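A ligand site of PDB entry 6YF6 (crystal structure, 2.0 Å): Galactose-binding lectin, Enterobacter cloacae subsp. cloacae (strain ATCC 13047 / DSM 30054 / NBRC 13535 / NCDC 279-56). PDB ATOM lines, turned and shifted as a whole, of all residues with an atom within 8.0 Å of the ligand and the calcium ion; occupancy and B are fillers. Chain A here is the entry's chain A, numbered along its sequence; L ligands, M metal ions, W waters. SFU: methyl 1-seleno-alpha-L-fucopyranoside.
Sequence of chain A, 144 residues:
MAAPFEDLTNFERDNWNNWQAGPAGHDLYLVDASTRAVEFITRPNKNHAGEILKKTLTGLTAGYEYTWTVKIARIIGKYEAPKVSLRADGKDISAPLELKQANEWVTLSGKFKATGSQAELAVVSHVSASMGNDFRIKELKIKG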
ATOM      1  N   PHE A  40     -27.473  32.558  31.145  1.00  0.00           N
ATOM      2  CA  PHE A  40     -28.564  31.839  30.481  1.00  0.00           C
ATOM      3  C   PHE A  40     -28.519  30.398  30.973  1.00  0.00           C
ATOM      4  O   PHE A  40     -27.754  29.578  30.458  1.00  0.00           O
ATOM      5  CB  PHE A  40     -28.435  31.918  28.967  1.00  0.00           C
ATOM      6  CG  PHE A  40     -28.458  33.323  28.424  1.00  0.00           C
ATOM      7  CD1 PHE A  40     -27.342  34.134  28.489  1.00  0.00           C
ATOM      8  CD2 PHE A  40     -29.606  33.832  27.834  1.00  0.00           C
ATOM      9  CE1 PHE A  40     -27.357  35.423  27.991  1.00  0.00           C
ATOM     10  CE2 PHE A  40     -29.643  35.120  27.330  1.00  0.00           C
ATOM     11  CZ  PHE A  40     -28.516  35.924  27.406  1.00  0.00           C
ATOM     12  N   ILE A  41     -29.339  30.090  31.985  1.00  0.00           N
ATOM     13  CA  ILE A  41     -29.400  28.746  32.552  1.00  0.00           C
ATOM     14  C   ILE A  41     -30.463  27.872  31.891  1.00  0.00           C
ATOM     15  O   ILE A  41     -30.490  26.655  32.131  1.00  0.00           O
ATOM     16  CB  ILE A  41     -29.630  28.855  34.069  1.00  0.00           C
ATOM     17  CG1 ILE A  41     -29.143  27.588  34.788  1.00  0.00           C
ATOM     18  CG2 ILE A  41     -31.085  29.131  34.358  1.00  0.00           C
ATOM     19  CD1 ILE A  41     -27.634  27.389  34.731  1.00  0.00           C
ATOM     20  N   THR A  42     -31.341  28.456  31.071  1.00  0.00           N
ATOM     21  CA  THR A  42     -32.358  27.747  30.298  1.00  0.00           C
ATOM     22  C   THR A  42     -33.061  26.649  31.102  1.00  0.00           C
ATOM     23  O   THR A  42     -32.706  25.472  31.004  1.00  0.00           O
ATOM     24  CB  THR A  42     -31.753  27.171  29.019  1.00  0.00           C
ATOM     25  OG1 THR A  42     -30.658  26.299  29.333  1.00  0.00           O
ATOM     26  CG2 THR A  42     -31.245  28.297  28.142  1.00  0.00           C
ATOM     27  N   ARG A  43     -34.070  27.049  31.876  1.00  0.00           N
ATOM     28  CA  ARG A  43     -34.728  26.146  32.789  1.00  0.00           C
ATOM     29  C   ARG A  43     -35.565  25.114  32.037  1.00  0.00           C
ATOM     30  O   ARG A  43     -35.888  25.292  30.863  1.00  0.00           O
ATOM     31  CB  ARG A  43     -35.647  26.931  33.735  1.00  0.00           C
ATOM     32  CG  ARG A  43     -34.949  27.947  34.632  1.00  0.00           C
ATOM     33  CD  ARG A  43     -35.991  28.642  35.478  1.00  0.00           C
ATOM     34  NE  ARG A  43     -35.501  29.776  36.244  1.00  0.00           N
ATOM     35  CZ  ARG A  43     -36.267  30.496  37.062  1.00  0.00           C
ATOM     36  NH1 ARG A  43     -37.552  30.178  37.210  1.00  0.00           N
ATOM     37  NH2 ARG A  43     -35.766  31.521  37.734  1.00  0.00           N
ATOM     38  N   PRO A  44     -35.952  24.015  32.714  1.00  0.00           N
ATOM     39  CA  PRO A  44     -36.709  22.963  32.031  1.00  0.00           C
ATOM     40  C   PRO A  44     -38.038  23.451  31.474  1.00  0.00           C
ATOM     41  O   PRO A  44     -38.694  24.324  32.038  1.00  0.00           O
ATOM     42  CB  PRO A  44     -36.932  21.924  33.148  1.00  0.00           C
ATOM     43  CG  PRO A  44     -35.843  22.180  34.140  1.00  0.00           C
ATOM     44  CD  PRO A  44     -35.599  23.654  34.101  1.00  0.00           C
ATOM     45  N   ASN A  45     -38.407  22.875  30.327  1.00  0.00           N
ATOM     46  CA  ASN A  45     -39.756  22.990  29.775  1.00  0.00           C
ATOM     47  C   ASN A  45     -40.117  24.413  29.381  1.00  0.00           C
ATOM     48  O   ASN A  45     -41.273  24.832  29.506  1.00  0.00           O
ATOM     49  CB  ASN A  45     -40.801  22.436  30.744  1.00  0.00           C
ATOM     50  CG  ASN A  45     -40.630  20.949  30.985  1.00  0.00           C
ATOM     51  OD1 ASN A  45     -40.023  20.243  30.164  1.00  0.00           O
ATOM     52  ND2 ASN A  45     -41.164  20.462  32.092  1.00  0.00           N
ATOM     53  N   HIS A  48     -36.148  27.857  24.469  1.00  0.00           N
ATOM     54  CA  HIS A  48     -35.046  28.810  24.520  1.00  0.00           C
ATOM     55  C   HIS A  48     -34.471  29.134  23.140  1.00  0.00           C
ATOM     56  O   HIS A  48     -33.367  29.674  23.042  1.00  0.00           O
ATOM     57  CB  HIS A  48     -33.949  28.283  25.442  1.00  0.00           C
ATOM     58  CG  HIS A  48     -34.480  27.838  26.775  1.00  0.00           C
ATOM     59  ND1 HIS A  48     -34.837  28.733  27.757  1.00  0.00           N
ATOM     60  CD2 HIS A  48     -34.751  26.610  27.267  1.00  0.00           C
ATOM     61  CE1 HIS A  48     -35.293  28.078  28.808  1.00  0.00           C
ATOM     62  NE2 HIS A  48     -35.249  26.781  28.538  1.00  0.00           N
ATOM     63  N   ARG A  74     -19.775  29.383  26.765  1.00  0.00           N
ATOM     64  CA  ARG A  74     -20.528  28.286  27.335  1.00  0.00           C
ATOM     65  C   ARG A  74     -20.122  28.096  28.792  1.00  0.00           C
ATOM     66  O   ARG A  74     -18.993  28.379  29.186  1.00  0.00           O
ATOM     67  CB  ARG A  74     -20.288  26.996  26.556  1.00  0.00           C
ATOM     68  CG  ARG A  74     -21.225  25.864  26.976  1.00  0.00           C
ATOM     69  CD  ARG A  74     -20.823  24.555  26.353  1.00  0.00           C
ATOM     70  NE  ARG A  74     -21.891  23.570  26.454  1.00  0.00           N
ATOM     71  CZ  ARG A  74     -21.822  22.338  25.951  1.00  0.00           C
ATOM     72  NH1 ARG A  74     -20.725  21.936  25.309  1.00  0.00           N
ATOM     73  NH2 ARG A  74     -22.851  21.510  26.089  1.00  0.00           N
ATOM     74  N   ILE A  75     -21.068  27.620  29.596  1.00  0.00           N
ATOM     75  CA  ILE A  75     -20.773  27.222  30.965  1.00  0.00           C
ATOM     76  C   ILE A  75     -21.255  25.785  31.165  1.00  0.00           C
ATOM     77  O   ILE A  75     -22.082  25.266  30.417  1.00  0.00           O
ATOM     78  CB  ILE A  75     -21.412  28.157  32.010  1.00  0.00           C
ATOM     79  CG1 ILE A  75     -22.929  28.227  31.828  1.00  0.00           C
ATOM     80  CG2 ILE A  75     -20.781  29.542  31.906  1.00  0.00           C
ATOM     81  CD1 ILE A  75     -23.665  28.721  33.063  1.00  0.00           C
ATOM     82  N   ILE A  76     -20.701  25.142  32.199  1.00  0.00           N
ATOM     83  CA  ILE A  76     -21.075  23.789  32.592  1.00  0.00           C
ATOM     84  C   ILE A  76     -20.573  22.793  31.565  1.00  0.00           C
ATOM     85  O   ILE A  76     -19.828  21.860  31.895  1.00  0.00           O
ATOM     86  CB  ILE A  76     -22.600  23.675  32.800  1.00  0.00           C
ATOM     87  CG1 ILE A  76     -23.052  24.703  33.841  1.00  0.00           C
ATOM     88  CG2 ILE A  76     -22.970  22.271  33.219  1.00  0.00           C
ATOM     89  CD1 ILE A  76     -24.549  24.767  34.059  1.00  0.00           C
ATOM     90  N   GLY A  77     -20.978  22.969  30.302  1.00  0.00           N
ATOM     91  CA  GLY A  77     -20.464  22.138  29.232  1.00  0.00           C
ATOM     92  C   GLY A  77     -21.128  20.797  29.068  1.00  0.00           C
ATOM     93  O   GLY A  77     -20.558  19.906  28.420  1.00  0.00           O
ATOM     94  N   LYS A  78     -22.322  20.608  29.620  1.00  0.00           N
ATOM     95  CA  LYS A  78     -22.980  19.318  29.589  1.00  0.00           C
ATOM     96  C   LYS A  78     -24.224  19.375  28.711  1.00  0.00           C
ATOM     97  O   LYS A  78     -24.883  20.410  28.597  1.00  0.00           O
ATOM     98  CB  LYS A  78     -23.343  18.861  31.006  1.00  0.00           C
ATOM     99  CG  LYS A  78     -22.203  18.136  31.719  1.00  0.00           C
ATOM    100  CD  LYS A  78     -22.655  17.426  32.981  1.00  0.00           C
ATOM    101  CE  LYS A  78     -23.861  16.526  32.747  1.00  0.00           C
ATOM    102  NZ  LYS A  78     -23.714  15.174  33.333  1.00  0.00           N
ATOM    103  N   TYR A  79     -24.529  18.236  28.113  1.00  0.00           N
ATOM    104  CA  TYR A  79     -25.726  18.061  27.268  1.00  0.00           C
ATOM    105  C   TYR A  79     -25.573  18.996  26.058  1.00  0.00           C
ATOM    106  O   TYR A  79     -24.490  19.077  25.479  1.00  0.00           O
ATOM    107  CB  TYR A  79     -26.957  18.277  28.122  1.00  0.00           C
ATOM    108  CG  TYR A  79     -27.053  17.295  29.273  1.00  0.00           C
ATOM    109  CD1 TYR A  79     -27.388  17.714  30.551  1.00  0.00           C
ATOM    110  CD2 TYR A  79     -26.808  15.938  29.076  1.00  0.00           C
ATOM    111  CE1 TYR A  79     -27.470  16.811  31.603  1.00  0.00           C
ATOM    112  CE2 TYR A  79     -26.888  15.038  30.120  1.00  0.00           C
ATOM    113  CZ  TYR A  79     -27.223  15.472  31.381  1.00  0.00           C
ATOM    114  OH  TYR A  79     -27.301  14.576  32.416  1.00  0.00           O
ATOM    115  N   GLU A  80     -26.629  19.703  25.658  1.00  0.00           N
ATOM    116  CA  GLU A  80     -26.633  20.372  24.371  1.00  0.00           C
ATOM    117  C   GLU A  80     -25.773  21.632  24.389  1.00  0.00           C
ATOM    118  O   GLU A  80     -25.799  22.419  25.338  1.00  0.00           O
ATOM    119  CB  GLU A  80     -28.058  20.715  23.954  1.00  0.00           C
ATOM    120  CG  GLU A  80     -28.774  19.558  23.263  1.00  0.00           C
ATOM    121  CD  GLU A  80     -29.879  20.018  22.335  1.00  0.00           C
ATOM    122  OE1 GLU A  80     -31.043  19.655  22.574  1.00  0.00           O
ATOM    123  OE2 GLU A  80     -29.568  20.731  21.357  1.00  0.00           O
ATOM    124  N   ALA A 129     -33.538  23.616  23.587  1.00  0.00           N
ATOM    125  CA  ALA A 129     -33.455  22.660  24.674  1.00  0.00           C
ATOM    126  C   ALA A 129     -33.148  23.341  26.001  1.00  0.00           C
ATOM    127  O   ALA A 129     -32.540  24.418  26.058  1.00  0.00           O
ATOM    128  CB  ALA A 129     -32.367  21.623  24.381  1.00  0.00           C
ATOM    129  N   SER A 130     -33.577  22.697  27.085  1.00  0.00           N
ATOM    130  CA  SER A 130     -33.205  23.096  28.441  1.00  0.00           C
ATOM    131  C   SER A 130     -32.097  22.241  29.018  1.00  0.00           C
ATOM    132  O   SER A 130     -31.316  22.723  29.851  1.00  0.00           O
ATOM    133  CB  SER A 130     -34.429  23.032  29.365  1.00  0.00           C
ATOM    134  OG  SER A 130     -34.816  21.684  29.569  1.00  0.00           O
ATOM    135  N   MET A 131     -31.994  20.983  28.580  1.00  0.00           N
ATOM    136  CA  MET A 131     -30.899  20.105  28.979  1.00  0.00           C
ATOM    137  C   MET A 131     -29.593  20.656  28.430  1.00  0.00           C
ATOM    138  O   MET A 131     -29.340  20.574  27.218  1.00  0.00           O
ATOM    139  CB  MET A 131     -31.150  18.689  28.475  1.00  0.00           C
ATOM    140  CG  MET A 131     -32.261  17.942  29.197  1.00  0.00           C
ATOM    141  SD  MET A 131     -31.808  17.501  30.889  1.00  0.00           S
ATOM    142  CE  MET A 131     -30.583  16.225  30.605  1.00  0.00           C
ATOM    143  N   GLY A 132     -28.766  21.224  29.298  1.00  0.00           N
ATOM    144  CA  GLY A 132     -27.598  21.942  28.855  1.00  0.00           C
ATOM    145  C   GLY A 132     -27.983  23.297  28.285  1.00  0.00           C
ATOM    146  O   GLY A 132     -28.857  23.972  28.837  1.00  0.00           O
ATOM    147  N   ASN A 133     -27.355  23.698  27.192  1.00  0.00           N
ATOM    148  CA  ASN A 133     -27.662  24.974  26.557  1.00  0.00           C
ATOM    149  C   ASN A 133     -27.499  26.129  27.555  1.00  0.00           C
ATOM    150  O   ASN A 133     -28.352  27.009  27.662  1.00  0.00           O
ATOM    151  CB  ASN A 133     -29.076  24.953  25.969  1.00  0.00           C
ATOM    152  CG  ASN A 133     -29.327  26.097  25.022  1.00  0.00           C
ATOM    153  OD1 ASN A 133     -28.399  26.651  24.442  1.00  0.00           O
ATOM    154  ND2 ASN A 133     -30.588  26.465  24.856  1.00  0.00           N
ATOM    155  N   ASP A 134     -26.395  26.101  28.297  1.00  0.00           N
ATOM    156  CA  ASP A 134     -26.097  27.069  29.346  1.00  0.00           C
ATOM    157  C   ASP A 134     -24.900  27.921  28.941  1.00  0.00           C
ATOM    158  O   ASP A 134     -23.861  27.391  28.544  1.00  0.00           O
ATOM    159  CB  ASP A 134     -25.812  26.364  30.671  1.00  0.00           C
ATOM    160  CG  ASP A 134     -26.899  25.361  31.036  1.00  0.00           C
ATOM    161  OD1 ASP A 134     -28.060  25.783  31.193  1.00  0.00           O
ATOM    162  OD2 ASP A 134     -26.579  24.163  31.163  1.00  0.00           O
ATOM    163  N   PHE A 135     -25.025  29.240  29.066  1.00  0.00           N
ATOM    164  CA  PHE A 135     -23.979  30.136  28.605  1.00  0.00           C
ATOM    165  C   PHE A 135     -24.152  31.498  29.264  1.00  0.00           C
ATOM    166  O   PHE A 135     -25.150  31.779  29.928  1.00  0.00           O
ATOM    167  CB  PHE A 135     -23.983  30.262  27.074  1.00  0.00           C
ATOM    168  CG  PHE A 135     -25.317  30.654  26.490  1.00  0.00           C
ATOM    169  CD1 PHE A 135     -26.339  29.726  26.349  1.00  0.00           C
ATOM    170  CD2 PHE A 135     -25.540  31.957  26.064  1.00  0.00           C
ATOM    171  CE1 PHE A 135     -27.559  30.092  25.796  1.00  0.00           C
ATOM    172  CE2 PHE A 135     -26.754  32.323  25.524  1.00  0.00           C
ATOM    173  CZ  PHE A 135     -27.762  31.393  25.385  1.00  0.00           C
HETATM  174  C1  SFU L   1     -30.466  20.237  33.228  1.00  0.00           C
HETATM  175  C2  SFU L   1     -31.106  21.614  33.074  1.00  0.00           C
HETATM  176  C3  SFU L   1     -30.227  22.751  33.635  1.00  0.00           C
HETATM  177  C4  SFU L   1     -28.840  22.632  33.014  1.00  0.00           C
HETATM  178  C5  SFU L   1     -28.290  21.253  33.352  1.00  0.00           C
HETATM  179  C6  SFU L   1     -26.907  21.093  32.736  1.00  0.00           C
HETATM  180  O2  SFU L   1     -32.354  21.611  33.740  1.00  0.00           O
HETATM  181  O3  SFU L   1     -30.760  23.998  33.216  1.00  0.00           O
HETATM  182  O4  SFU L   1     -28.892  22.737  31.606  1.00  0.00           O
HETATM  183  O5  SFU L   1     -29.116  20.197  32.815  1.00  0.00           O
HETATM  184  CM  SFU L   1     -29.614  18.016  35.074  1.00  0.00           C
HETATM  185 SE   SFU L   1     -30.595  19.655  35.143  1.00  0.00          SE
HETATM  186 CA    CA M   1     -30.224  24.639  30.890  1.00  0.00          CA
HETATM  187  O   HOH W   1     -33.989  20.075  31.602  1.00  0.00           O
HETATM  188  O   HOH W   2     -32.260  25.218  35.129  1.00  0.00           O
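Water W1 lies within hydrogen-bond range of OG of Ser 130 (2.7 Å), O2 of the ligand (3.1 Å) and SD of Met 131 (3.4 Å).
The backbone NH (N) of Gly 132 lies close to an oxygen (O4) of the ligand (2.8 Å).
The side-chain hydroxyl (OG1) of Thr 42 is bound to the calcium ion (2.3 Å). O of Ile 41 is bound to the calcium ion, at 2.4 Å. An oxygen (O4) of the ligand is bound to the calcium ion (2.4 Å). The calcium ion is bound by O of Ser 130. The side-chain carboxylate (OD1) of Asp 134 is bound to the calcium ion (2.5 Å). The calcium ion is bound by O3 of the ligand, at 2.5 Å. The backbone carbonyl oxygen (O) of Gly 132 binds the calcium ion (2.6 Å). The backbone carbonyl oxygen (O) of Thr 42 binds the calcium ion, 2.6 Å away.
Within 4 Å of the calcium ion: Ile 41, Thr 42, Ser 130, Gly 132 and Asp 134.
Pro 44 touches the ligand (CG to O2, 3.6 Å). Tyr 79 touches the ligand. Met 131 touches the ligand (SD to C1, 3.8 Å). Hydrophobic or aromatic side chains within 4 Å of the ligand: Pro 44, Tyr 79 and Met 131. Within 4 Å of the ligand: Ile 41, Thr 42, Pro 44, Tyr 79, Ser 130, Met 131, Gly 132 and Asp 134.
O of Tyr 79 is in hydrogen-bond range of NH2 of Arg 74, at 3.0 Å. The side-chain hydroxyl (OG1) of Thr 42 lies close to the backbone carbonyl oxygen (O) of Asn 133, 2.9 Å away. The backbone NH (N) of Ile 75 sits at hydrogen-bond distance from the backbone carbonyl oxygen (O) of Asp 134. The backbone NH (N) of Glu 80 sits at hydrogen-bond distance from the backbone carbonyl oxygen (O) of Met 131 (3.2 Å).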
